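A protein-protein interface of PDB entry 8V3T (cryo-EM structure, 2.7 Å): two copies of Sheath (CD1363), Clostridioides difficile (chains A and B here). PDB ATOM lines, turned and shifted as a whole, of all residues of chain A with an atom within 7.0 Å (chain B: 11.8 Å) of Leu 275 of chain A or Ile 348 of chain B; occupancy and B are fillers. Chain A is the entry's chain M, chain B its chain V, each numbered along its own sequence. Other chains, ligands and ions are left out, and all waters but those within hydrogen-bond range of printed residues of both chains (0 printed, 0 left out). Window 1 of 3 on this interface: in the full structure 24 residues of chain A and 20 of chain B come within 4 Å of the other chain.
No position is printed for both chains.
The backbone NH (N) of Ser 351 of chain B sits at hydrogen-bond distance from the backbone carbonyl oxygen (O) of Leu 335 of chain A (3.1 Å).
The backbone carbonyl oxygen (O) of Val 333 of chain A is in hydrogen-bond range of the backbone NH (N) of Asp 349 of chain B (2.8 Å).
The side-chain carboxylate of Asp 343 of chain B lies within hydrogen-bond range of the side-chain hydroxyl of Ser 331 of chain A (2.9 Å).
The side-chain amino group (NZ) of Lys 332 of chain A lies within salt-bridge range of the side-chain carboxylate (OD2) of Asp 347 of chain B (3.5 Å).
O of Asp 347 of chain B lies within hydrogen-bond range of N of Val 333 of chain A (3.0 Å).
The backbone carbonyl oxygen (O) of Ser 331 of chain A lies within hydrogen-bond range of the backbone NH (N) of Asp 347 of chain B.
The side-chain hydroxyl of Ser 331 of chain A sits at hydrogen-bond distance from the backbone carbonyl oxygen of Ala 344 of chain B, 3.0 Å away.
The backbone NH of Leu 335 of chain A sits at hydrogen-bond distance from the backbone carbonyl oxygen of Asp 349 of chain B, 2.8 Å away.
Printed residues of chain B that touch a printed residue of chain A: Asp 343, Ala 344, Met 345, Glu 346, Asp 347, Ile 348, Asp 349, Leu 350 and Ser 351.
Hydrophobic or aromatic side chains of chain B within 4 Å of the printed part of chain A: Met 345, Ile 348 and Leu 350.
Hydrophobic or aromatic side chains of chain A within 4 Å of the printed part of chain B: Ile 257, Ile 262, Leu 275, Val 333 and Leu 335.
Among the printed residues, 19 pairs touch across the chains.
Among the printed residues, Asp or Glu carboxylates within 4 Å of a Lys or Arg side-chain nitrogen of the other chain: Lys 332 of chain A with Asp 347 of chain B (3.5 Å).
Ile 257 of chain A touches Ile 348 of chain B (CG2 to CD1, 3.7 Å).
Met 345 of chain B touches Tyr 261 of chain A.
CA of Ile 262 of chain A touches O of Met 345 of chain B (3.5 Å).
Ile 262 of chain A touches Glu 346 of chain B.
Met 345 of chain B touches Asn 271 of chain A (CE to CB, 3.7 Å).
CD2 of Leu 275 of chain A touches CD1 of Ile 348 of chain B, 3.7 Å away.
Glu 346 of chain B touches Ser 331 of chain A (N to O, 3.5 Å).
CG2 of Val 333 of chain A touches CG of Met 345 of chain B, at 3.6 Å.
Ile 348 of chain B touches Val 333 of chain A (CA to O, 3.5 Å).
Leu 335 of chain A touches Leu 350 of chain B (O to CA, 3.3 Å).
Ile 257 of chain A touches just one residue of chain B: Ile 348.
Asp 270 of chain A touches none of the printed residues of chain B.
Lys 272 of chain A touches none of the printed residues of chain B.
No residue of chain B comes within 4 Å of Cys 273 of chain A.
Of chain B, only Ile 348 comes within 4 Å of Leu 275 of chain A.
No residue of chain B comes within 4 Å of Ile 276 of chain A.
Val 277 of chain A touches none of the printed residues of chain B.
Val 333 of chain A touches four residues of chain B.
Leu 335 of chain A touches just these residues of chain B: Asp 349 (2.8 Å), Leu 350 (3.3 Å) and Ser 351 (3.1 Å).
Of the printed residues of chain A, Ala 344 of chain B touches Ser 331.
Of chain A, only Ile 257 (3.7 Å), Leu 275 (3.7 Å) and Val 333 (3.5 Å) come within 4 Å of Ile 348 of chain B.
Of the printed residues of chain A, Asp 349 of chain B touches Val 333 (2.8 Å), Phe 334 (3.5 Å) and Leu 335 (2.8 Å).
The nearest residue of chain A that does not touch Ile 348 of chain B is Ile 262 of chain A (4.7 Å).
The nearest printed residue of chain B that does not touch Phe 334 of chain A is Ile 348 of chain B (5.7 Å).
The backbone NH of Ile 262 of chain A is in hydrogen-bond range of the backbone carbonyl oxygen of Ile 257 of chain A, 3.5 Å away.
OE2 of Glu 346 of chain B sits at hydrogen-bond distance from OG1 of Thr 181 of chain B (3.0 Å).
The side-chain carboxylate of Asp 347 of chain B lies within salt-bridge range of the guanidinium group of Arg 221 of chain B (3.8 Å).
NH1 of Arg 221 of chain B lies within salt-bridge range of OE1 of Glu 346 of chain B, at 2.6 Å.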
ATOM      1  N   VAL A 256     -21.435  12.769  -3.027  1.00  0.00           N
ATOM      2  CA  VAL A 256     -21.047  13.224  -1.689  1.00  0.00           C
ATOM      3  C   VAL A 256     -21.916  12.559  -0.626  1.00  0.00           C
ATOM      4  O   VAL A 256     -21.410  12.068   0.398  1.00  0.00           O
ATOM      5  CB  VAL A 256     -21.086  14.762  -1.571  1.00  0.00           C
ATOM      6  CG1 VAL A 256     -22.024  15.372  -2.570  1.00  0.00           C
ATOM      7  CG2 VAL A 256     -21.458  15.191  -0.155  1.00  0.00           C
ATOM      8  N   ILE A 257     -23.233  12.502  -0.862  1.00  0.00           N
ATOM      9  CA  ILE A 257     -24.142  11.941   0.136  1.00  0.00           C
ATOM     10  C   ILE A 257     -23.796  10.484   0.417  1.00  0.00           C
ATOM     11  O   ILE A 257     -23.733  10.054   1.575  1.00  0.00           O
ATOM     12  CB  ILE A 257     -25.605  12.094  -0.317  1.00  0.00           C
ATOM     13  CG1 ILE A 257     -26.030  13.562  -0.268  1.00  0.00           C
ATOM     14  CG2 ILE A 257     -26.521  11.246   0.545  1.00  0.00           C
ATOM     15  CD1 ILE A 257     -27.493  13.781  -0.579  1.00  0.00           C
ATOM     16  N   TYR A 261     -22.277  10.022   4.327  1.00  0.00           N
ATOM     17  CA  TYR A 261     -23.382  10.058   5.280  1.00  0.00           C
ATOM     18  C   TYR A 261     -24.256   8.813   5.341  1.00  0.00           C
ATOM     19  O   TYR A 261     -24.895   8.598   6.379  1.00  0.00           O
ATOM     20  CB  TYR A 261     -24.281  11.272   5.003  1.00  0.00           C
ATOM     21  CG  TYR A 261     -23.592  12.584   5.288  1.00  0.00           C
ATOM     22  CD1 TYR A 261     -22.842  13.223   4.311  1.00  0.00           C
ATOM     23  CD2 TYR A 261     -23.675  13.175   6.539  1.00  0.00           C
ATOM     24  CE1 TYR A 261     -22.201  14.415   4.570  1.00  0.00           C
ATOM     25  CE2 TYR A 261     -23.038  14.369   6.807  1.00  0.00           C
ATOM     26  CZ  TYR A 261     -22.303  14.984   5.820  1.00  0.00           C
ATOM     27  OH  TYR A 261     -21.668  16.173   6.081  1.00  0.00           O
ATOM     28  N   ILE A 262     -24.316   7.987   4.301  1.00  0.00           N
ATOM     29  CA  ILE A 262     -25.217   6.837   4.311  1.00  0.00           C
ATOM     30  C   ILE A 262     -24.616   5.758   5.206  1.00  0.00           C
ATOM     31  O   ILE A 262     -23.587   5.165   4.877  1.00  0.00           O
ATOM     32  CB  ILE A 262     -25.475   6.307   2.898  1.00  0.00           C
ATOM     33  CG1 ILE A 262     -26.133   7.386   2.038  1.00  0.00           C
ATOM     34  CG2 ILE A 262     -26.350   5.065   2.954  1.00  0.00           C
ATOM     35  CD1 ILE A 262     -27.568   7.670   2.411  1.00  0.00           C
ATOM     36  N   TYR A 269     -30.770  15.891  14.493  1.00  0.00           N
ATOM     37  CA  TYR A 269     -30.894  17.220  13.902  1.00  0.00           C
ATOM     38  C   TYR A 269     -29.529  17.852  13.645  1.00  0.00           C
ATOM     39  O   TYR A 269     -29.337  18.548  12.640  1.00  0.00           O
ATOM     40  CB  TYR A 269     -31.745  18.110  14.808  1.00  0.00           C
ATOM     41  CG  TYR A 269     -32.191  19.396  14.157  1.00  0.00           C
ATOM     42  CD1 TYR A 269     -33.020  19.378  13.045  1.00  0.00           C
ATOM     43  CD2 TYR A 269     -31.788  20.626  14.653  1.00  0.00           C
ATOM     44  CE1 TYR A 269     -33.431  20.547  12.445  1.00  0.00           C
ATOM     45  CE2 TYR A 269     -32.194  21.801  14.059  1.00  0.00           C
ATOM     46  CZ  TYR A 269     -33.016  21.755  12.956  1.00  0.00           C
ATOM     47  OH  TYR A 269     -33.426  22.924  12.359  1.00  0.00           O
ATOM     48  N   ASP A 270     -28.570  17.623  14.544  1.00  0.00           N
ATOM     49  CA  ASP A 270     -27.232  18.181  14.373  1.00  0.00           C
ATOM     50  C   ASP A 270     -26.567  17.646  13.108  1.00  0.00           C
ATOM     51  O   ASP A 270     -25.959  18.401  12.336  1.00  0.00           O
ATOM     52  CB  ASP A 270     -26.384  17.864  15.604  1.00  0.00           C
ATOM     53  CG  ASP A 270     -26.909  18.530  16.860  1.00  0.00           C
ATOM     54  OD1 ASP A 270     -27.788  19.407  16.746  1.00  0.00           O
ATOM     55  OD2 ASP A 270     -26.448  18.170  17.963  1.00  0.00           O
ATOM     56  N   ASN A 271     -26.675  16.337  12.879  1.00  0.00           N
ATOM     57  CA  ASN A 271     -26.098  15.747  11.678  1.00  0.00           C
ATOM     58  C   ASN A 271     -26.814  16.232  10.424  1.00  0.00           C
ATOM     59  O   ASN A 271     -26.182  16.398   9.373  1.00  0.00           O
ATOM     60  CB  ASN A 271     -26.145  14.225  11.776  1.00  0.00           C
ATOM     61  CG  ASN A 271     -25.184  13.680  12.812  1.00  0.00           C
ATOM     62  OD1 ASN A 271     -24.159  14.291  13.107  1.00  0.00           O
ATOM     63  ND2 ASN A 271     -25.513  12.524  13.374  1.00  0.00           N
ATOM     64  N   LYS A 272     -28.123  16.472  10.516  1.00  0.00           N
ATOM     65  CA  LYS A 272     -28.846  17.065   9.398  1.00  0.00           C
ATOM     66  C   LYS A 272     -28.310  18.453   9.077  1.00  0.00           C
ATOM     67  O   LYS A 272     -28.148  18.810   7.904  1.00  0.00           O
ATOM     68  CB  LYS A 272     -30.341  17.125   9.712  1.00  0.00           C
ATOM     69  CG  LYS A 272     -31.011  15.767   9.804  1.00  0.00           C
ATOM     70  CD  LYS A 272     -32.510  15.904  10.001  1.00  0.00           C
ATOM     71  CE  LYS A 272     -33.151  14.558  10.283  1.00  0.00           C
ATOM     72  NZ  LYS A 272     -34.584  14.693  10.658  1.00  0.00           N
ATOM     73  N   CYS A 273     -28.028  19.252  10.110  1.00  0.00           N
ATOM     74  CA  CYS A 273     -27.448  20.574   9.887  1.00  0.00           C
ATOM     75  C   CYS A 273     -26.075  20.473   9.232  1.00  0.00           C
ATOM     76  O   CYS A 273     -25.742  21.264   8.340  1.00  0.00           O
ATOM     77  CB  CYS A 273     -27.362  21.334  11.210  1.00  0.00           C
ATOM     78  SG  CYS A 273     -28.962  21.805  11.899  1.00  0.00           S
ATOM     79  N   LEU A 274     -25.261  19.508   9.668  1.00  0.00           N
ATOM     80  CA  LEU A 274     -23.949  19.320   9.052  1.00  0.00           C
ATOM     81  C   LEU A 274     -24.076  18.946   7.576  1.00  0.00           C
ATOM     82  O   LEU A 274     -23.330  19.453   6.725  1.00  0.00           O
ATOM     83  CB  LEU A 274     -23.164  18.253   9.815  1.00  0.00           C
ATOM     84  CG  LEU A 274     -22.632  18.662  11.189  1.00  0.00           C
ATOM     85  CD1 LEU A 274     -22.107  17.458  11.951  1.00  0.00           C
ATOM     86  CD2 LEU A 274     -21.551  19.719  11.052  1.00  0.00           C
ATOM     87  N   LEU A 275     -25.022  18.059   7.256  1.00  0.00           N
ATOM     88  CA  LEU A 275     -25.265  17.695   5.864  1.00  0.00           C
ATOM     89  C   LEU A 275     -25.714  18.902   5.045  1.00  0.00           C
ATOM     90  O   LEU A 275     -25.283  19.084   3.897  1.00  0.00           O
ATOM     91  CB  LEU A 275     -26.309  16.581   5.800  1.00  0.00           C
ATOM     92  CG  LEU A 275     -26.822  16.143   4.429  1.00  0.00           C
ATOM     93  CD1 LEU A 275     -25.682  15.657   3.554  1.00  0.00           C
ATOM     94  CD2 LEU A 275     -27.875  15.064   4.589  1.00  0.00           C
ATOM     95  N   ILE A 276     -26.588  19.731   5.620  1.00  0.00           N
ATOM     96  CA  ILE A 276     -27.034  20.945   4.941  1.00  0.00           C
ATOM     97  C   ILE A 276     -25.846  21.847   4.639  1.00  0.00           C
ATOM     98  O   ILE A 276     -25.742  22.419   3.547  1.00  0.00           O
ATOM     99  CB  ILE A 276     -28.092  21.675   5.789  1.00  0.00           C
ATOM    100  CG1 ILE A 276     -29.389  20.869   5.843  1.00  0.00           C
ATOM    101  CG2 ILE A 276     -28.360  23.063   5.239  1.00  0.00           C
ATOM    102  CD1 ILE A 276     -30.504  21.578   6.568  1.00  0.00           C
ATOM    103  N   VAL A 277     -24.935  21.990   5.603  1.00  0.00           N
ATOM    104  CA  VAL A 277     -23.757  22.830   5.403  1.00  0.00           C
ATOM    105  C   VAL A 277     -22.897  22.290   4.265  1.00  0.00           C
ATOM    106  O   VAL A 277     -22.402  23.050   3.423  1.00  0.00           O
ATOM    107  CB  VAL A 277     -22.959  22.947   6.714  1.00  0.00           C
ATOM    108  CG1 VAL A 277     -21.565  23.486   6.451  1.00  0.00           C
ATOM    109  CG2 VAL A 277     -23.699  23.831   7.701  1.00  0.00           C
ATOM    110  N   ALA A 278     -22.703  20.969   4.222  1.00  0.00           N
ATOM    111  CA  ALA A 278     -21.901  20.381   3.149  1.00  0.00           C
ATOM    112  C   ALA A 278     -22.528  20.639   1.780  1.00  0.00           C
ATOM    113  O   ALA A 278     -21.837  21.022   0.821  1.00  0.00           O
ATOM    114  CB  ALA A 278     -21.726  18.882   3.389  1.00  0.00           C
ATOM    115  N   ILE A 279     -23.844  20.439   1.671  1.00  0.00           N
ATOM    116  CA  ILE A 279     -24.522  20.659   0.394  1.00  0.00           C
ATOM    117  C   ILE A 279     -24.434  22.126  -0.013  1.00  0.00           C
ATOM    118  O   ILE A 279     -24.223  22.451  -1.191  1.00  0.00           O
ATOM    119  CB  ILE A 279     -25.981  20.177   0.474  1.00  0.00           C
ATOM    120  CG1 ILE A 279     -26.029  18.680   0.786  1.00  0.00           C
ATOM    121  CG2 ILE A 279     -26.710  20.467  -0.826  1.00  0.00           C
ATOM    122  CD1 ILE A 279     -27.427  18.117   0.862  1.00  0.00           C
ATOM    123  N   LYS A 280     -24.597  23.034   0.951  1.00  0.00           N
ATOM    124  CA  LYS A 280     -24.496  24.458   0.654  1.00  0.00           C
ATOM    125  C   LYS A 280     -23.102  24.822   0.161  1.00  0.00           C
ATOM    126  O   LYS A 280     -22.954  25.637  -0.757  1.00  0.00           O
ATOM    127  CB  LYS A 280     -24.860  25.276   1.893  1.00  0.00           C
ATOM    128  CG  LYS A 280     -24.809  26.778   1.684  1.00  0.00           C
ATOM    129  CD  LYS A 280     -25.751  27.206   0.575  1.00  0.00           C
ATOM    130  CE  LYS A 280     -25.577  28.675   0.239  1.00  0.00           C
ATOM    131  NZ  LYS A 280     -25.992  29.550   1.369  1.00  0.00           N
ATOM    132  N   SER A 281     -22.065  24.238   0.765  1.00  0.00           N
ATOM    133  CA  SER A 281     -20.706  24.505   0.308  1.00  0.00           C
ATOM    134  C   SER A 281     -20.505  24.027  -1.125  1.00  0.00           C
ATOM    135  O   SER A 281     -19.880  24.721  -1.942  1.00  0.00           O
ATOM    136  CB  SER A 281     -19.694  23.839   1.240  1.00  0.00           C
ATOM    137  OG  SER A 281     -19.856  22.433   1.245  1.00  0.00           O
ATOM    138  N   VAL A 298     -30.303  26.157   0.653  1.00  0.00           N
ATOM    139  CA  VAL A 298     -30.647  24.813   1.104  1.00  0.00           C
ATOM    140  C   VAL A 298     -31.206  24.921   2.515  1.00  0.00           C
ATOM    141  O   VAL A 298     -30.706  25.709   3.326  1.00  0.00           O
ATOM    142  CB  VAL A 298     -29.434  23.856   1.085  1.00  0.00           C
ATOM    143  CG1 VAL A 298     -29.898  22.410   1.091  1.00  0.00           C
ATOM    144  CG2 VAL A 298     -28.540  24.124  -0.112  1.00  0.00           C
ATOM    145  N   SER A 331     -35.142   6.925   9.919  1.00  0.00           N
ATOM    146  CA  SER A 331     -34.027   6.942   8.983  1.00  0.00           C
ATOM    147  C   SER A 331     -34.202   7.951   7.856  1.00  0.00           C
ATOM    148  O   SER A 331     -33.359   7.999   6.955  1.00  0.00           O
ATOM    149  CB  SER A 331     -33.819   5.546   8.388  1.00  0.00           C
ATOM    150  OG  SER A 331     -32.992   4.754   9.220  1.00  0.00           O
ATOM    151  N   LYS A 332     -35.260   8.753   7.880  1.00  0.00           N
ATOM    152  CA  LYS A 332     -35.558   9.665   6.786  1.00  0.00           C
ATOM    153  C   LYS A 332     -34.982  11.054   7.041  1.00  0.00           C
ATOM    154  O   LYS A 332     -34.895  11.514   8.182  1.00  0.00           O
ATOM    155  CB  LYS A 332     -37.068   9.770   6.568  1.00  0.00           C
ATOM    156  CG  LYS A 332     -37.786   8.437   6.484  1.00  0.00           C
ATOM    157  CD  LYS A 332     -37.486   7.741   5.170  1.00  0.00           C
ATOM    158  CE  LYS A 332     -38.485   6.632   4.887  1.00  0.00           C
ATOM    159  NZ  LYS A 332     -38.268   5.454   5.768  1.00  0.00           N
ATOM    160  N   VAL A 333     -34.586  11.714   5.955  1.00  0.00           N
ATOM    161  CA  VAL A 333     -34.162  13.109   5.966  1.00  0.00           C
ATOM    162  C   VAL A 333     -34.877  13.822   4.829  1.00  0.00           C
ATOM    163  O   VAL A 333     -34.911  13.317   3.702  1.00  0.00           O
ATOM    164  CB  VAL A 333     -32.634  13.254   5.819  1.00  0.00           C
ATOM    165  CG1 VAL A 333     -32.228  14.714   5.916  1.00  0.00           C
ATOM    166  CG2 VAL A 333     -31.913  12.433   6.869  1.00  0.00           C
ATOM    167  N   PHE A 334     -35.446  14.989   5.120  1.00  0.00           N
ATOM    168  CA  PHE A 334     -36.188  15.772   4.138  1.00  0.00           C
ATOM    169  C   PHE A 334     -35.530  17.135   3.983  1.00  0.00           C
ATOM    170  O   PHE A 334     -35.403  17.880   4.959  1.00  0.00           O
ATOM    171  CB  PHE A 334     -37.653  15.927   4.554  1.00  0.00           C
ATOM    172  CG  PHE A 334     -38.347  14.623   4.820  1.00  0.00           C
ATOM    173  CD1 PHE A 334     -38.963  13.931   3.794  1.00  0.00           C
ATOM    174  CD2 PHE A 334     -38.385  14.091   6.097  1.00  0.00           C
ATOM    175  CE1 PHE A 334     -39.603  12.734   4.035  1.00  0.00           C
ATOM    176  CE2 PHE A 334     -39.022  12.893   6.343  1.00  0.00           C
ATOM    177  CZ  PHE A 334     -39.632  12.214   5.310  1.00  0.00           C
ATOM    178  N   LEU A 335     -35.121  17.457   2.758  1.00  0.00           N
ATOM    179  CA  LEU A 335     -34.473  18.722   2.450  1.00  0.00           C
ATOM    180  C   LEU A 335     -35.056  19.298   1.167  1.00  0.00           C
ATOM    181  O   LEU A 335     -35.618  18.579   0.338  1.00  0.00           O
ATOM    182  CB  LEU A 335     -32.954  18.560   2.296  1.00  0.00           C
ATOM    183  CG  LEU A 335     -32.204  17.804   3.392  1.00  0.00           C
ATOM    184  CD1 LEU A 335     -30.779  17.521   2.962  1.00  0.00           C
ATOM    185  CD2 LEU A 335     -32.226  18.590   4.691  1.00  0.00           C
ATOM    186  N   THR B 181     -25.021  -0.886   6.050  1.00  0.00           N
ATOM    187  CA  THR B 181     -25.774  -0.517   4.860  1.00  0.00           C
ATOM    188  C   THR B 181     -24.886   0.242   3.880  1.00  0.00           C
ATOM    189  O   THR B 181     -24.185   1.185   4.260  1.00  0.00           O
ATOM    190  CB  THR B 181     -26.986   0.332   5.245  1.00  0.00           C
ATOM    191  OG1 THR B 181     -27.849  -0.430   6.097  1.00  0.00           O
ATOM    192  CG2 THR B 181     -27.758   0.753   4.006  1.00  0.00           C
ATOM    193  N   TYR B 182     -24.911  -0.186   2.617  1.00  0.00           N
ATOM    194  CA  TYR B 182     -24.143   0.414   1.528  1.00  0.00           C
ATOM    195  C   TYR B 182     -22.638   0.341   1.758  1.00  0.00           C
ATOM    196  O   TYR B 182     -21.884   1.149   1.206  1.00  0.00           O
ATOM    197  CB  TYR B 182     -24.568   1.865   1.275  1.00  0.00           C
ATOM    198  CG  TYR B 182     -25.603   2.015   0.185  1.00  0.00           C
ATOM    199  CD1 TYR B 182     -26.710   1.179   0.132  1.00  0.00           C
ATOM    200  CD2 TYR B 182     -25.473   2.990  -0.793  1.00  0.00           C
ATOM    201  CE1 TYR B 182     -27.657   1.311  -0.863  1.00  0.00           C
ATOM    202  CE2 TYR B 182     -26.416   3.131  -1.792  1.00  0.00           C
ATOM    203  CZ  TYR B 182     -27.505   2.288  -1.822  1.00  0.00           C
ATOM    204  OH  TYR B 182     -28.449   2.425  -2.814  1.00  0.00           O
ATOM    205  N   ARG B 221     -28.946  -3.704   2.337  1.00  0.00           N
ATOM    206  CA  ARG B 221     -29.546  -3.278   3.591  1.00  0.00           C
ATOM    207  C   ARG B 221     -29.040  -4.186   4.702  1.00  0.00           C
ATOM    208  O   ARG B 221     -28.656  -5.333   4.458  1.00  0.00           O
ATOM    209  CB  ARG B 221     -31.078  -3.309   3.506  1.00  0.00           C
ATOM    210  CG  ARG B 221     -31.803  -2.718   4.704  1.00  0.00           C
ATOM    211  CD  ARG B 221     -31.741  -1.202   4.691  1.00  0.00           C
ATOM    212  NE  ARG B 221     -33.065  -0.605   4.573  1.00  0.00           N
ATOM    213  CZ  ARG B 221     -33.289   0.677   4.321  1.00  0.00           C
ATOM    214  NH1 ARG B 221     -32.294   1.532   4.152  1.00  0.00           N
ATOM    215  NH2 ARG B 221     -34.543   1.113   4.240  1.00  0.00           N
ATOM    216  N   ASP B 343     -31.273   5.418  15.256  1.00  0.00           N
ATOM    217  CA  ASP B 343     -30.922   4.693  14.044  1.00  0.00           C
ATOM    218  C   ASP B 343     -30.030   5.563  13.166  1.00  0.00           C
ATOM    219  O   ASP B 343     -29.910   6.774  13.368  1.00  0.00           O
ATOM    220  CB  ASP B 343     -32.181   4.265  13.278  1.00  0.00           C
ATOM    221  CG  ASP B 343     -31.910   3.163  12.274  1.00  0.00           C
ATOM    222  OD1 ASP B 343     -30.817   2.562  12.327  1.00  0.00           O
ATOM    223  OD2 ASP B 343     -32.793   2.895  11.433  1.00  0.00           O
ATOM    224  N   ALA B 344     -29.395   4.930  12.186  1.00  0.00           N
ATOM    225  CA  ALA B 344     -28.481   5.625  11.293  1.00  0.00           C
ATOM    226  C   ALA B 344     -29.242   6.317  10.164  1.00  0.00           C
ATOM    227  O   ALA B 344     -30.450   6.140   9.985  1.00  0.00           O
ATOM    228  CB  ALA B 344     -27.449   4.654  10.722  1.00  0.00           C
ATOM    229  N   MET B 345     -28.511   7.121   9.395  1.00  0.00           N
ATOM    230  CA  MET B 345     -29.066   7.834   8.250  1.00  0.00           C
ATOM    231  C   MET B 345     -29.001   6.937   7.022  1.00  0.00           C
ATOM    232  O   MET B 345     -27.909   6.541   6.595  1.00  0.00           O
ATOM    233  CB  MET B 345     -28.294   9.129   8.003  1.00  0.00           C
ATOM    234  CG  MET B 345     -29.152  10.376   7.932  1.00  0.00           C
ATOM    235  SD  MET B 345     -28.186  11.850   7.542  1.00  0.00           S
ATOM    236  CE  MET B 345     -28.210  12.703   9.115  1.00  0.00           C
ATOM    237  N   GLU B 346     -30.161   6.612   6.452  1.00  0.00           N
ATOM    238  CA  GLU B 346     -30.196   5.737   5.283  1.00  0.00           C
ATOM    239  C   GLU B 346     -31.051   6.244   4.127  1.00  0.00           C
ATOM    240  O   GLU B 346     -30.773   5.870   2.984  1.00  0.00           O
ATOM    241  CB  GLU B 346     -30.678   4.336   5.681  1.00  0.00           C
ATOM    242  CG  GLU B 346     -29.675   3.551   6.513  1.00  0.00           C
ATOM    243  CD  GLU B 346     -30.191   2.185   6.923  1.00  0.00           C
ATOM    244  OE1 GLU B 346     -31.311   1.822   6.507  1.00  0.00           O
ATOM    245  OE2 GLU B 346     -29.477   1.473   7.659  1.00  0.00           O
ATOM    246  N   ASP B 347     -32.070   7.068   4.362  1.00  0.00           N
ATOM    247  CA  ASP B 347     -32.957   7.544   3.308  1.00  0.00           C
ATOM    248  C   ASP B 347     -32.978   9.064   3.305  1.00  0.00           C
ATOM    249  O   ASP B 347     -33.112   9.689   4.362  1.00  0.00           O
ATOM    250  CB  ASP B 347     -34.372   6.993   3.493  1.00  0.00           C
ATOM    251  CG  ASP B 347     -34.422   5.483   3.424  1.00  0.00           C
ATOM    252  OD1 ASP B 347     -33.709   4.907   2.578  1.00  0.00           O
ATOM    253  OD2 ASP B 347     -35.170   4.872   4.213  1.00  0.00           O
ATOM    254  N   ILE B 348     -32.849   9.656   2.119  1.00  0.00           N
ATOM    255  CA  ILE B 348     -32.789  11.105   1.967  1.00  0.00           C
ATOM    256  C   ILE B 348     -33.690  11.520   0.812  1.00  0.00           C
ATOM    257  O   ILE B 348     -33.635  10.925  -0.268  1.00  0.00           O
ATOM    258  CB  ILE B 348     -31.346  11.592   1.726  1.00  0.00           C
ATOM    259  CG1 ILE B 348     -30.495  11.365   2.976  1.00  0.00           C
ATOM    260  CG2 ILE B 348     -31.333  13.059   1.325  1.00  0.00           C
ATOM    261  CD1 ILE B 348     -29.165  12.066   2.945  1.00  0.00           C
ATOM    262  N   ASP B 349     -34.515  12.539   1.040  1.00  0.00           N
ATOM    263  CA  ASP B 349     -35.322  13.159  -0.002  1.00  0.00           C
ATOM    264  C   ASP B 349     -34.918  14.621  -0.129  1.00  0.00           C
ATOM    265  O   ASP B 349     -34.943  15.361   0.859  1.00  0.00           O
ATOM    266  CB  ASP B 349     -36.817  13.046   0.309  1.00  0.00           C
ATOM    267  CG  ASP B 349     -37.388  11.690  -0.053  1.00  0.00           C
ATOM    268  OD1 ASP B 349     -36.868  10.670   0.445  1.00  0.00           O
ATOM    269  OD2 ASP B 349     -38.358  11.641  -0.837  1.00  0.00           O
ATOM    270  N   LEU B 350     -34.553  15.033  -1.341  1.00  0.00           N
ATOM    271  CA  LEU B 350     -34.110  16.397  -1.605  1.00  0.00           C
ATOM    272  C   LEU B 350     -34.833  16.916  -2.837  1.00  0.00           C
ATOM    273  O   LEU B 350     -34.645  16.388  -3.938  1.00  0.00           O
ATOM    274  CB  LEU B 350     -32.591  16.453  -1.801  1.00  0.00           C
ATOM    275  CG  LEU B 350     -31.998  17.728  -2.403  1.00  0.00           C
ATOM    276  CD1 LEU B 350     -32.042  18.869  -1.406  1.00  0.00           C
ATOM    277  CD2 LEU B 350     -30.574  17.483  -2.871  1.00  0.00           C
ATOM    278  N   SER B 351     -35.649  17.950  -2.653  1.00  0.00           N
ATOM    279  CA  SER B 351     -36.446  18.538  -3.721  1.00  0.00           C
ATOM    280  C   SER B 351     -35.815  19.860  -4.134  1.00  0.00           C
ATOM    281  O   SER B 351     -35.583  20.731  -3.290  1.00  0.00           O
ATOM    282  CB  SER B 351     -37.891  18.746  -3.270  1.00  0.00           C
ATOM    283  OG  SER B 351     -38.709  19.153  -4.352  1.00  0.00           O
ATOM    284  N   ILE B 352     -35.541  20.009  -5.426  1.00  0.00           N
ATOM    285  CA  ILE B 352     -34.852  21.178  -5.960  1.00  0.00           C
ATOM    286  C   ILE B 352     -35.790  21.905  -6.910  1.00  0.00           C
ATOM    287  O   ILE B 352     -36.376  21.288  -7.807  1.00  0.00           O
ATOM    288  CB  ILE B 352     -33.545  20.788  -6.672  1.00  0.00           C
ATOM    289  CG1 ILE B 352     -32.663  19.957  -5.742  1.00  0.00           C
ATOM    290  CG2 ILE B 352     -32.808  22.027  -7.148  1.00  0.00           C
ATOM    291  CD1 ILE B 352     -31.333  19.581  -6.341  1.00  0.00           C
